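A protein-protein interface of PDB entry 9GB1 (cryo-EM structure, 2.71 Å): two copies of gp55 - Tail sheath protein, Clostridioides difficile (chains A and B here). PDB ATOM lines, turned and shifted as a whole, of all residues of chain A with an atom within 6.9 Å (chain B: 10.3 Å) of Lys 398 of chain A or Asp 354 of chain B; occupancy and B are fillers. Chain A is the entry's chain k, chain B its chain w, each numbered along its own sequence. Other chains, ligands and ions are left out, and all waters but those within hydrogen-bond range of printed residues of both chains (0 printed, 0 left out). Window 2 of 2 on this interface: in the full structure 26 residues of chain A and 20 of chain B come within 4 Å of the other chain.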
ATOM      1  N   ARG A 223     -20.378  -8.972  30.139  1.00  0.00           N
ATOM      2  CA  ARG A 223     -19.864 -10.338  30.210  1.00  0.00           C
ATOM      3  C   ARG A 223     -20.991 -11.355  30.335  1.00  0.00           C
ATOM      4  O   ARG A 223     -21.036 -12.339  29.592  1.00  0.00           O
ATOM      5  CB  ARG A 223     -18.904 -10.472  31.397  1.00  0.00           C
ATOM      6  CG  ARG A 223     -17.602  -9.692  31.269  1.00  0.00           C
ATOM      7  CD  ARG A 223     -16.729  -9.886  32.506  1.00  0.00           C
ATOM      8  NE  ARG A 223     -15.483  -9.127  32.448  1.00  0.00           N
ATOM      9  CZ  ARG A 223     -14.580  -9.077  33.419  1.00  0.00           C
ATOM     10  NH1 ARG A 223     -14.717  -9.778  34.536  1.00  0.00           N
ATOM     11  NH2 ARG A 223     -13.510  -8.300  33.271  1.00  0.00           N
ATOM     12  N   SER A 225     -25.303 -12.446  31.669  1.00  0.00           N
ATOM     13  CA  SER A 225     -26.720 -12.142  31.529  1.00  0.00           C
ATOM     14  C   SER A 225     -27.336 -11.973  32.911  1.00  0.00           C
ATOM     15  O   SER A 225     -26.948 -12.663  33.858  1.00  0.00           O
ATOM     16  CB  SER A 225     -27.447 -13.255  30.770  1.00  0.00           C
ATOM     17  OG  SER A 225     -26.946 -13.387  29.451  1.00  0.00           O
ATOM     18  N   SER A 394     -34.920 -18.794  23.229  1.00  0.00           N
ATOM     19  CA  SER A 394     -33.688 -18.337  22.602  1.00  0.00           C
ATOM     20  C   SER A 394     -32.459 -19.095  23.083  1.00  0.00           C
ATOM     21  O   SER A 394     -31.423 -19.040  22.411  1.00  0.00           O
ATOM     22  CB  SER A 394     -33.506 -16.841  22.849  1.00  0.00           C
ATOM     23  OG  SER A 394     -34.606 -16.111  22.335  1.00  0.00           O
ATOM     24  N   LEU A 395     -32.538 -19.798  24.218  1.00  0.00           N
ATOM     25  CA  LEU A 395     -31.448 -20.681  24.617  1.00  0.00           C
ATOM     26  C   LEU A 395     -31.365 -21.938  23.764  1.00  0.00           C
ATOM     27  O   LEU A 395     -30.348 -22.636  23.826  1.00  0.00           O
ATOM     28  CB  LEU A 395     -31.586 -21.099  26.084  1.00  0.00           C
ATOM     29  CG  LEU A 395     -31.438 -20.043  27.180  1.00  0.00           C
ATOM     30  CD1 LEU A 395     -31.758 -20.639  28.542  1.00  0.00           C
ATOM     31  CD2 LEU A 395     -30.036 -19.459  27.162  1.00  0.00           C
ATOM     32  N   LYS A 396     -32.390 -22.237  22.971  1.00  0.00           N
ATOM     33  CA  LYS A 396     -32.392 -23.433  22.131  1.00  0.00           C
ATOM     34  C   LYS A 396     -31.656 -23.188  20.814  1.00  0.00           C
ATOM     35  O   LYS A 396     -32.197 -23.457  19.761  1.00  0.00           O
ATOM     36  CB  LYS A 396     -33.823 -23.875  21.835  1.00  0.00           C
ATOM     37  CG  LYS A 396     -34.709 -24.280  22.993  1.00  0.00           C
ATOM     38  CD  LYS A 396     -34.248 -25.580  23.620  1.00  0.00           C
ATOM     39  CE  LYS A 396     -35.144 -25.981  24.774  1.00  0.00           C
ATOM     40  NZ  LYS A 396     -36.503 -26.354  24.280  1.00  0.00           N
ATOM     41  N   ARG A 397     -30.420 -22.679  20.867  1.00  0.00           N
ATOM     42  CA  ARG A 397     -29.581 -22.596  19.668  1.00  0.00           C
ATOM     43  C   ARG A 397     -28.289 -23.375  19.768  1.00  0.00           C
ATOM     44  O   ARG A 397     -27.606 -23.528  18.748  1.00  0.00           O
ATOM     45  CB  ARG A 397     -29.210 -21.151  19.308  1.00  0.00           C
ATOM     46  CG  ARG A 397     -30.353 -20.304  18.840  1.00  0.00           C
ATOM     47  CD  ARG A 397     -29.858 -18.975  18.288  1.00  0.00           C
ATOM     48  NE  ARG A 397     -29.197 -18.108  19.256  1.00  0.00           N
ATOM     49  CZ  ARG A 397     -29.801 -17.214  20.030  1.00  0.00           C
ATOM     50  NH1 ARG A 397     -31.111 -17.019  19.985  1.00  0.00           N
ATOM     51  NH2 ARG A 397     -29.067 -16.476  20.856  1.00  0.00           N
ATOM     52  N   LYS A 398     -27.929 -23.875  20.943  1.00  0.00           N
ATOM     53  CA  LYS A 398     -26.603 -24.448  21.118  1.00  0.00           C
ATOM     54  C   LYS A 398     -26.495 -25.830  20.479  1.00  0.00           C
ATOM     55  O   LYS A 398     -25.388 -26.369  20.382  1.00  0.00           O
ATOM     56  CB  LYS A 398     -26.236 -24.504  22.606  1.00  0.00           C
ATOM     57  CG  LYS A 398     -26.844 -23.400  23.511  1.00  0.00           C
ATOM     58  CD  LYS A 398     -26.638 -21.963  23.003  1.00  0.00           C
ATOM     59  CE  LYS A 398     -27.297 -20.963  23.945  1.00  0.00           C
ATOM     60  NZ  LYS A 398     -27.314 -19.573  23.405  1.00  0.00           N
ATOM     61  N   GLU A 399     -27.625 -26.413  20.056  1.00  0.00           N
ATOM     62  CA  GLU A 399     -27.673 -27.721  19.415  1.00  0.00           C
ATOM     63  C   GLU A 399     -28.660 -27.742  18.251  1.00  0.00           C
ATOM     64  O   GLU A 399     -28.978 -28.818  17.734  1.00  0.00           O
ATOM     65  CB  GLU A 399     -28.033 -28.788  20.461  1.00  0.00           C
ATOM     66  CG  GLU A 399     -29.409 -28.605  21.151  1.00  0.00           C
ATOM     67  CD  GLU A 399     -30.589 -29.213  20.402  1.00  0.00           C
ATOM     68  OE1 GLU A 399     -30.388 -30.099  19.547  1.00  0.00           O
ATOM     69  OE2 GLU A 399     -31.734 -28.799  20.683  1.00  0.00           O
ATOM     70  N   PHE A 400     -29.105 -26.569  17.799  1.00  0.00           N
ATOM     71  CA  PHE A 400     -30.409 -26.455  17.164  1.00  0.00           C
ATOM     72  C   PHE A 400     -30.370 -25.649  15.868  1.00  0.00           C
ATOM     73  O   PHE A 400     -31.099 -25.957  14.922  1.00  0.00           O
ATOM     74  CB  PHE A 400     -31.329 -25.789  18.165  1.00  0.00           C
ATOM     75  CG  PHE A 400     -32.736 -25.641  17.718  1.00  0.00           C
ATOM     76  CD1 PHE A 400     -33.588 -26.724  17.724  1.00  0.00           C
ATOM     77  CD2 PHE A 400     -33.208 -24.428  17.268  1.00  0.00           C
ATOM     78  CE1 PHE A 400     -34.881 -26.573  17.340  1.00  0.00           C
ATOM     79  CE2 PHE A 400     -34.492 -24.289  16.887  1.00  0.00           C
ATOM     80  CZ  PHE A 400     -35.322 -25.345  16.919  1.00  0.00           C
ATOM     81  N   VAL A 401     -29.542 -24.604  15.825  1.00  0.00           N
ATOM     82  CA  VAL A 401     -29.395 -23.730  14.662  1.00  0.00           C
ATOM     83  C   VAL A 401     -28.076 -24.053  13.982  1.00  0.00           C
ATOM     84  O   VAL A 401     -27.021 -24.062  14.629  1.00  0.00           O
ATOM     85  CB  VAL A 401     -29.458 -22.242  15.046  1.00  0.00           C
ATOM     86  CG1 VAL A 401     -29.190 -21.378  13.828  1.00  0.00           C
ATOM     87  CG2 VAL A 401     -30.822 -21.899  15.603  1.00  0.00           C
ATOM     88  N   LYS A 403     -27.445 -26.948  12.954  1.00  0.00           N
ATOM     89  CA  LYS A 403     -27.199 -28.333  13.303  1.00  0.00           C
ATOM     90  C   LYS A 403     -28.430 -29.206  13.066  1.00  0.00           C
ATOM     91  O   LYS A 403     -28.401 -30.393  13.408  1.00  0.00           O
ATOM     92  CB  LYS A 403     -26.773 -28.416  14.776  1.00  0.00           C
ATOM     93  CG  LYS A 403     -25.407 -27.784  15.128  1.00  0.00           C
ATOM     94  CD  LYS A 403     -25.154 -27.990  16.618  1.00  0.00           C
ATOM     95  CE  LYS A 403     -23.856 -27.397  17.141  1.00  0.00           C
ATOM     96  NZ  LYS A 403     -23.746 -27.665  18.605  1.00  0.00           N
ATOM     97  N   LYS B 314     -15.494 -30.413  10.288  1.00  0.00           N
ATOM     98  CA  LYS B 314     -16.853 -30.525   9.777  1.00  0.00           C
ATOM     99  C   LYS B 314     -16.842 -30.985   8.328  1.00  0.00           C
ATOM    100  O   LYS B 314     -17.589 -31.897   7.954  1.00  0.00           O
ATOM    101  CB  LYS B 314     -17.581 -29.186   9.905  1.00  0.00           C
ATOM    102  CG  LYS B 314     -17.753 -28.675  11.332  1.00  0.00           C
ATOM    103  CD  LYS B 314     -18.694 -29.557  12.141  1.00  0.00           C
ATOM    104  CE  LYS B 314     -18.916 -28.997  13.531  1.00  0.00           C
ATOM    105  NZ  LYS B 314     -19.795 -29.868  14.354  1.00  0.00           N
ATOM    106  N   SER B 319     -21.159 -27.391   9.285  1.00  0.00           N
ATOM    107  CA  SER B 319     -20.854 -25.985   9.074  1.00  0.00           C
ATOM    108  C   SER B 319     -20.469 -25.389  10.417  1.00  0.00           C
ATOM    109  O   SER B 319     -20.721 -25.982  11.469  1.00  0.00           O
ATOM    110  CB  SER B 319     -22.041 -25.237   8.461  1.00  0.00           C
ATOM    111  OG  SER B 319     -21.841 -23.837   8.503  1.00  0.00           O
ATOM    112  N   CYS B 321     -21.272 -22.085  11.289  1.00  0.00           N
ATOM    113  CA  CYS B 321     -21.986 -20.816  11.385  1.00  0.00           C
ATOM    114  C   CYS B 321     -22.169 -20.395  12.836  1.00  0.00           C
ATOM    115  O   CYS B 321     -21.922 -19.237  13.192  1.00  0.00           O
ATOM    116  CB  CYS B 321     -23.341 -20.923  10.685  1.00  0.00           C
ATOM    117  SG  CYS B 321     -24.345 -22.319  11.226  1.00  0.00           S
ATOM    118  N   ASN B 322     -22.614 -21.317  13.686  1.00  0.00           N
ATOM    119  CA  ASN B 322     -22.793 -21.066  15.113  1.00  0.00           C
ATOM    120  C   ASN B 322     -22.291 -22.255  15.916  1.00  0.00           C
ATOM    121  O   ASN B 322     -22.940 -22.708  16.865  1.00  0.00           O
ATOM    122  CB  ASN B 322     -24.259 -20.773  15.449  1.00  0.00           C
ATOM    123  CG  ASN B 322     -24.797 -19.472  14.819  1.00  0.00           C
ATOM    124  OD1 ASN B 322     -26.011 -19.333  14.670  1.00  0.00           O
ATOM    125  ND2 ASN B 322     -23.926 -18.509  14.502  1.00  0.00           N
ATOM    126  N   ALA B 323     -21.127 -22.778  15.545  1.00  0.00           N
ATOM    127  CA  ALA B 323     -20.563 -23.916  16.252  1.00  0.00           C
ATOM    128  C   ALA B 323     -20.050 -23.496  17.624  1.00  0.00           C
ATOM    129  O   ALA B 323     -19.587 -22.369  17.824  1.00  0.00           O
ATOM    130  CB  ALA B 323     -19.432 -24.543  15.441  1.00  0.00           C
ATOM    131  N   LYS B 324     -20.134 -24.423  18.573  1.00  0.00           N
ATOM    132  CA  LYS B 324     -19.716 -24.182  19.952  1.00  0.00           C
ATOM    133  C   LYS B 324     -18.194 -24.255  20.011  1.00  0.00           C
ATOM    134  O   LYS B 324     -17.600 -25.324  20.171  1.00  0.00           O
ATOM    135  CB  LYS B 324     -20.378 -25.188  20.889  1.00  0.00           C
ATOM    136  CG  LYS B 324     -20.672 -24.649  22.283  1.00  0.00           C
ATOM    137  CD  LYS B 324     -21.478 -25.632  23.141  1.00  0.00           C
ATOM    138  CE  LYS B 324     -20.749 -26.946  23.419  1.00  0.00           C
ATOM    139  NZ  LYS B 324     -19.486 -26.744  24.180  1.00  0.00           N
ATOM    140  N   THR B 325     -17.550 -23.102  19.866  1.00  0.00           N
ATOM    141  CA  THR B 325     -16.096 -23.054  19.919  1.00  0.00           C
ATOM    142  C   THR B 325     -15.616 -23.157  21.362  1.00  0.00           C
ATOM    143  O   THR B 325     -16.305 -22.753  22.303  1.00  0.00           O
ATOM    144  CB  THR B 325     -15.561 -21.768  19.283  1.00  0.00           C
ATOM    145  OG1 THR B 325     -15.741 -20.675  20.187  1.00  0.00           O
ATOM    146  CG2 THR B 325     -16.273 -21.462  17.970  1.00  0.00           C
ATOM    147  N   ILE B 326     -14.413 -23.710  21.530  1.00  0.00           N
ATOM    148  CA  ILE B 326     -13.873 -23.928  22.870  1.00  0.00           C
ATOM    149  C   ILE B 326     -13.493 -22.624  23.561  1.00  0.00           C
ATOM    150  O   ILE B 326     -13.312 -22.611  24.784  1.00  0.00           O
ATOM    151  CB  ILE B 326     -12.641 -24.860  22.848  1.00  0.00           C
ATOM    152  CG1 ILE B 326     -11.624 -24.431  21.783  1.00  0.00           C
ATOM    153  CG2 ILE B 326     -13.076 -26.294  22.600  1.00  0.00           C
ATOM    154  CD1 ILE B 326     -10.211 -24.858  22.083  1.00  0.00           C
ATOM    155  N   PHE B 327     -13.357 -21.529  22.816  1.00  0.00           N
ATOM    156  CA  PHE B 327     -12.889 -20.282  23.404  1.00  0.00           C
ATOM    157  C   PHE B 327     -13.912 -19.742  24.393  1.00  0.00           C
ATOM    158  O   PHE B 327     -15.122 -19.888  24.201  1.00  0.00           O
ATOM    159  CB  PHE B 327     -12.606 -19.252  22.312  1.00  0.00           C
ATOM    160  CG  PHE B 327     -11.701 -19.758  21.228  1.00  0.00           C
ATOM    161  CD1 PHE B 327     -10.387 -20.099  21.502  1.00  0.00           C
ATOM    162  CD2 PHE B 327     -12.173 -19.916  19.940  1.00  0.00           C
ATOM    163  CE1 PHE B 327      -9.559 -20.572  20.507  1.00  0.00           C
ATOM    164  CE2 PHE B 327     -11.352 -20.389  18.944  1.00  0.00           C
ATOM    165  CZ  PHE B 327     -10.042 -20.718  19.225  1.00  0.00           C
ATOM    166  N   GLU B 328     -13.412 -19.144  25.476  1.00  0.00           N
ATOM    167  CA  GLU B 328     -14.249 -18.653  26.564  1.00  0.00           C
ATOM    168  C   GLU B 328     -14.387 -17.133  26.595  1.00  0.00           C
ATOM    169  O   GLU B 328     -15.100 -16.616  27.460  1.00  0.00           O
ATOM    170  CB  GLU B 328     -13.712 -19.168  27.911  1.00  0.00           C
ATOM    171  CG  GLU B 328     -12.287 -18.738  28.296  1.00  0.00           C
ATOM    172  CD  GLU B 328     -12.212 -17.388  28.995  1.00  0.00           C
ATOM    173  OE1 GLU B 328     -13.238 -16.918  29.532  1.00  0.00           O
ATOM    174  OE2 GLU B 328     -11.113 -16.796  29.014  1.00  0.00           O
ATOM    175  N   GLU B 329     -13.738 -16.402  25.686  1.00  0.00           N
ATOM    176  CA  GLU B 329     -13.930 -14.957  25.613  1.00  0.00           C
ATOM    177  C   GLU B 329     -13.374 -14.482  24.277  1.00  0.00           C
ATOM    178  O   GLU B 329     -12.415 -15.056  23.753  1.00  0.00           O
ATOM    179  CB  GLU B 329     -13.253 -14.251  26.807  1.00  0.00           C
ATOM    180  CG  GLU B 329     -13.662 -12.785  27.099  1.00  0.00           C
ATOM    181  CD  GLU B 329     -13.120 -11.722  26.147  1.00  0.00           C
ATOM    182  OE1 GLU B 329     -12.326 -12.027  25.241  1.00  0.00           O
ATOM    183  OE2 GLU B 329     -13.509 -10.547  26.317  1.00  0.00           O
ATOM    184  N   VAL B 330     -13.989 -13.427  23.730  1.00  0.00           N
ATOM    185  CA  VAL B 330     -13.594 -12.835  22.452  1.00  0.00           C
ATOM    186  C   VAL B 330     -13.665 -11.315  22.535  1.00  0.00           C
ATOM    187  O   VAL B 330     -14.151 -10.737  23.509  1.00  0.00           O
ATOM    188  CB  VAL B 330     -14.451 -13.329  21.263  1.00  0.00           C
ATOM    189  CG1 VAL B 330     -14.292 -14.810  21.068  1.00  0.00           C
ATOM    190  CG2 VAL B 330     -15.936 -12.974  21.467  1.00  0.00           C
ATOM    191  N   ARG B 333     -16.623  -6.353  20.052  1.00  0.00           N
ATOM    192  CA  ARG B 333     -18.038  -6.698  19.949  1.00  0.00           C
ATOM    193  C   ARG B 333     -18.780  -5.577  19.234  1.00  0.00           C
ATOM    194  O   ARG B 333     -18.307  -4.441  19.150  1.00  0.00           O
ATOM    195  CB  ARG B 333     -18.698  -6.953  21.320  1.00  0.00           C
ATOM    196  CG  ARG B 333     -18.431  -8.330  21.952  1.00  0.00           C
ATOM    197  CD  ARG B 333     -17.037  -8.486  22.547  1.00  0.00           C
ATOM    198  NE  ARG B 333     -16.844  -9.788  23.179  1.00  0.00           N
ATOM    199  CZ  ARG B 333     -17.139 -10.083  24.438  1.00  0.00           C
ATOM    200  NH1 ARG B 333     -17.728  -9.211  25.241  1.00  0.00           N
ATOM    201  NH2 ARG B 333     -16.845 -11.295  24.903  1.00  0.00           N
ATOM    202  N   LEU B 350     -16.226 -13.885  15.787  1.00  0.00           N
ATOM    203  CA  LEU B 350     -16.685 -14.695  16.902  1.00  0.00           C
ATOM    204  C   LEU B 350     -17.486 -13.835  17.871  1.00  0.00           C
ATOM    205  O   LEU B 350     -17.270 -12.624  17.984  1.00  0.00           O
ATOM    206  CB  LEU B 350     -15.499 -15.329  17.630  1.00  0.00           C
ATOM    207  CG  LEU B 350     -14.739 -16.467  16.945  1.00  0.00           C
ATOM    208  CD1 LEU B 350     -13.439 -16.756  17.674  1.00  0.00           C
ATOM    209  CD2 LEU B 350     -15.582 -17.719  16.912  1.00  0.00           C
ATOM    210  N   ASP B 351     -18.417 -14.476  18.575  1.00  0.00           N
ATOM    211  CA  ASP B 351     -19.260 -13.804  19.554  1.00  0.00           C
ATOM    212  C   ASP B 351     -19.381 -14.676  20.792  1.00  0.00           C
ATOM    213  O   ASP B 351     -19.340 -15.906  20.710  1.00  0.00           O
ATOM    214  CB  ASP B 351     -20.656 -13.502  18.998  1.00  0.00           C
ATOM    215  CG  ASP B 351     -20.638 -12.436  17.918  1.00  0.00           C
ATOM    216  OD1 ASP B 351     -19.747 -11.563  17.953  1.00  0.00           O
ATOM    217  OD2 ASP B 351     -21.522 -12.470  17.038  1.00  0.00           O
ATOM    218  N   PHE B 352     -19.540 -14.021  21.943  1.00  0.00           N
ATOM    219  CA  PHE B 352     -19.637 -14.708  23.228  1.00  0.00           C
ATOM    220  C   PHE B 352     -21.127 -14.761  23.559  1.00  0.00           C
ATOM    221  O   PHE B 352     -21.648 -13.993  24.367  1.00  0.00           O
ATOM    222  CB  PHE B 352     -18.829 -13.968  24.293  1.00  0.00           C
ATOM    223  CG  PHE B 352     -18.929 -14.564  25.668  1.00  0.00           C
ATOM    224  CD1 PHE B 352     -18.216 -15.711  25.977  1.00  0.00           C
ATOM    225  CD2 PHE B 352     -19.738 -14.008  26.639  1.00  0.00           C
ATOM    226  CE1 PHE B 352     -18.284 -16.271  27.235  1.00  0.00           C
ATOM    227  CE2 PHE B 352     -19.821 -14.578  27.894  1.00  0.00           C
ATOM    228  CZ  PHE B 352     -19.095 -15.707  28.191  1.00  0.00           C
ATOM    229  N   ASP B 353     -21.832 -15.671  22.883  1.00  0.00           N
ATOM    230  CA  ASP B 353     -23.288 -15.707  22.986  1.00  0.00           C
ATOM    231  C   ASP B 353     -23.753 -16.275  24.321  1.00  0.00           C
ATOM    232  O   ASP B 353     -24.790 -15.851  24.842  1.00  0.00           O
ATOM    233  CB  ASP B 353     -23.869 -16.522  21.830  1.00  0.00           C
ATOM    234  CG  ASP B 353     -25.313 -16.919  22.061  1.00  0.00           C
ATOM    235  OD1 ASP B 353     -26.115 -16.047  22.455  1.00  0.00           O
ATOM    236  OD2 ASP B 353     -25.647 -18.103  21.846  1.00  0.00           O
ATOM    237  N   ASP B 354     -23.008 -17.221  24.878  1.00  0.00           N
ATOM    238  CA  ASP B 354     -23.270 -17.763  26.207  1.00  0.00           C
ATOM    239  C   ASP B 354     -21.907 -17.932  26.868  1.00  0.00           C
ATOM    240  O   ASP B 354     -20.917 -17.344  26.423  1.00  0.00           O
ATOM    241  CB  ASP B 354     -24.103 -19.057  26.133  1.00  0.00           C
ATOM    242  CG  ASP B 354     -23.488 -20.114  25.232  1.00  0.00           C
ATOM    243  OD1 ASP B 354     -22.249 -20.209  25.131  1.00  0.00           O
ATOM    244  OD2 ASP B 354     -24.259 -20.883  24.634  1.00  0.00           O
ATOM    245  N   GLY B 355     -21.848 -18.734  27.937  1.00  0.00           N
ATOM    246  CA  GLY B 355     -20.592 -18.955  28.641  1.00  0.00           C
ATOM    247  C   GLY B 355     -19.447 -19.421  27.759  1.00  0.00           C
ATOM    248  O   GLY B 355     -18.277 -19.227  28.106  1.00  0.00           O
ATOM    249  N   ASP B 356     -19.756 -20.047  26.623  1.00  0.00           N
ATOM    250  CA  ASP B 356     -18.773 -20.424  25.617  1.00  0.00           C
ATOM    251  C   ASP B 356     -18.986 -19.625  24.336  1.00  0.00           C
ATOM    252  O   ASP B 356     -20.098 -19.190  24.027  1.00  0.00           O
ATOM    253  CB  ASP B 356     -18.840 -21.924  25.316  1.00  0.00           C
ATOM    254  CG  ASP B 356     -18.901 -22.768  26.573  1.00  0.00           C
ATOM    255  OD1 ASP B 356     -18.025 -22.594  27.446  1.00  0.00           O
ATOM    256  OD2 ASP B 356     -19.822 -23.603  26.689  1.00  0.00           O
ATOM    257  N   VAL B 357     -17.893 -19.426  23.602  1.00  0.00           N
ATOM    258  CA  VAL B 357     -17.920 -18.606  22.397  1.00  0.00           C
ATOM    259  C   VAL B 357     -18.647 -19.342  21.275  1.00  0.00           C
ATOM    260  O   VAL B 357     -18.613 -20.576  21.182  1.00  0.00           O
ATOM    261  CB  VAL B 357     -16.475 -18.238  22.008  1.00  0.00           C
ATOM    262  CG1 VAL B 357     -16.389 -17.622  20.613  1.00  0.00           C
ATOM    263  CG2 VAL B 357     -15.890 -17.283  23.035  1.00  0.00           C
ATOM    264  N   ILE B 358     -19.315 -18.573  20.412  1.00  0.00           N
ATOM    265  CA  ILE B 358     -20.055 -19.103  19.270  1.00  0.00           C
ATOM    266  C   ILE B 358     -19.791 -18.216  18.057  1.00  0.00           C
ATOM    267  O   ILE B 358     -19.779 -16.985  18.163  1.00  0.00           O
ATOM    268  CB  ILE B 358     -21.572 -19.202  19.561  1.00  0.00           C
ATOM    269  CG1 ILE B 358     -21.845 -20.192  20.709  1.00  0.00           C
ATOM    270  CG2 ILE B 358     -22.321 -19.593  18.284  1.00  0.00           C
ATOM    271  CD1 ILE B 358     -23.267 -20.182  21.270  1.00  0.00           C
ATOM    272  N   ILE B 359     -19.581 -18.853  16.899  1.00  0.00           N
ATOM    273  CA  ILE B 359     -19.381 -18.123  15.646  1.00  0.00           C
ATOM    274  C   ILE B 359     -20.685 -17.436  15.242  1.00  0.00           C
ATOM    275  O   ILE B 359     -21.789 -17.880  15.575  1.00  0.00           O
ATOM    276  CB  ILE B 359     -18.882 -19.085  14.550  1.00  0.00           C
ATOM    277  CG1 ILE B 359     -17.512 -19.670  14.932  1.00  0.00           C
ATOM    278  CG2 ILE B 359     -18.769 -18.358  13.197  1.00  0.00           C
ATOM    279  CD1 ILE B 359     -17.035 -20.830  14.082  1.00  0.00           C
ATOM    280  N   ILE B 466     -34.971 -18.429  12.608  1.00  0.00           N
ATOM    281  CA  ILE B 466     -36.183 -18.971  13.206  1.00  0.00           C
ATOM    282  C   ILE B 466     -36.903 -17.817  13.888  1.00  0.00           C
ATOM    283  O   ILE B 466     -36.299 -17.118  14.708  1.00  0.00           O
ATOM    284  CB  ILE B 466     -35.857 -20.097  14.209  1.00  0.00           C
ATOM    285  CG1 ILE B 466     -34.786 -21.036  13.621  1.00  0.00           C
ATOM    286  CG2 ILE B 466     -37.116 -20.869  14.587  1.00  0.00           C
ATOM    287  CD1 ILE B 466     -34.400 -22.164  14.478  1.00  0.00           C
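The guanidinium group (NH2) of Arg 397 of chain A is in salt-bridge range of the side-chain carboxylate (OD1) of Asp 353 of chain B, 3.4 Å away.
The side-chain amino group of Lys 398 of chain A lies within salt-bridge range of the side-chain carboxylate of Asp 353 of chain B, at 2.7 Å.
The side-chain amino group (NZ) of Lys 398 of chain A is in salt-bridge range of the side-chain carboxylate (OD2) of Asp 354 of chain B, at 3.5 Å.
The backbone carbonyl oxygen (O) of Ser 394 of chain A lies within hydrogen-bond range of the guanidinium group (NH1) of Arg 397 of chain A (3.2 Å).
O of Lys 398 of chain A is in hydrogen-bond range of NZ of Lys 403 of chain A.
ND2 of Asn 322 of chain B is in hydrogen-bond range of O of Ile 359 of chain B.
N of Asp 356 of chain B lies within hydrogen-bond range of OD1 of Asp 354 of chain B (2.9 Å).
Among the printed residues, pairs that only touch across the chains: Arg 223 of chain A with Phe 352 of chain B (3.1 Å), Phe 400 of chain A with Ile 466 of chain B (3.2 Å), Val 401 of chain A with Asn 322 of chain B (3.9 Å) and Val 401 of chain A with Ile 466 of chain B (3.8 Å).
Lys 398 of chain A touches two residues of chain B.
Asp 354 of chain B touches just one residue of chain A: Lys 398 (3.1 Å).
No residue of chain B comes within 4 Å of Glu 399 of chain A.
Printed residues of chain A within 4 Å of Ile 466 of chain B: Phe 400 (3.2 Å) and Val 401 (3.8 Å).
Of the printed residues of chain A, Asn 322 of chain B touches Val 401 (3.9 Å).
Of the printed residues of chain A, Phe 352 of chain B touches Arg 223.
Cys 321 of chain B touches none of the printed residues of chain A.
Thr 325 of chain B touches none of the printed residues of chain A.
The nearest residue of chain A that does not touch Asp 354 of chain B is Arg 223 of chain A (5.9 Å).
Printed residues of chain A that touch a printed residue of chain B: Arg 223, Arg 397, Lys 398, Phe 400 and Val 401.
Hydrophobic or aromatic side chains of chain A that line the printed part of chain B: Phe 400 and Val 401.
Printed residues of chain B that touch a printed residue of chain A: Asn 322, Phe 352, Asp 353, Asp 354 and Ile 466.
Among the printed residues, 7 pairs touch across the chains.
Among the printed residues, Asp or Glu carboxylates within 4 Å of a Lys or Arg side-chain nitrogen of the other chain: Arg 397 of chain A with Asp 353 of chain B, Lys 398 of chain A with Asp 353 of chain B and Lys 398 of chain A with Asp 354 of chain B.
No position is printed for both chains.
Of the 7 pairs that touch across the chains among the printed residues, none has its exchanged pair printed and touching as well.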
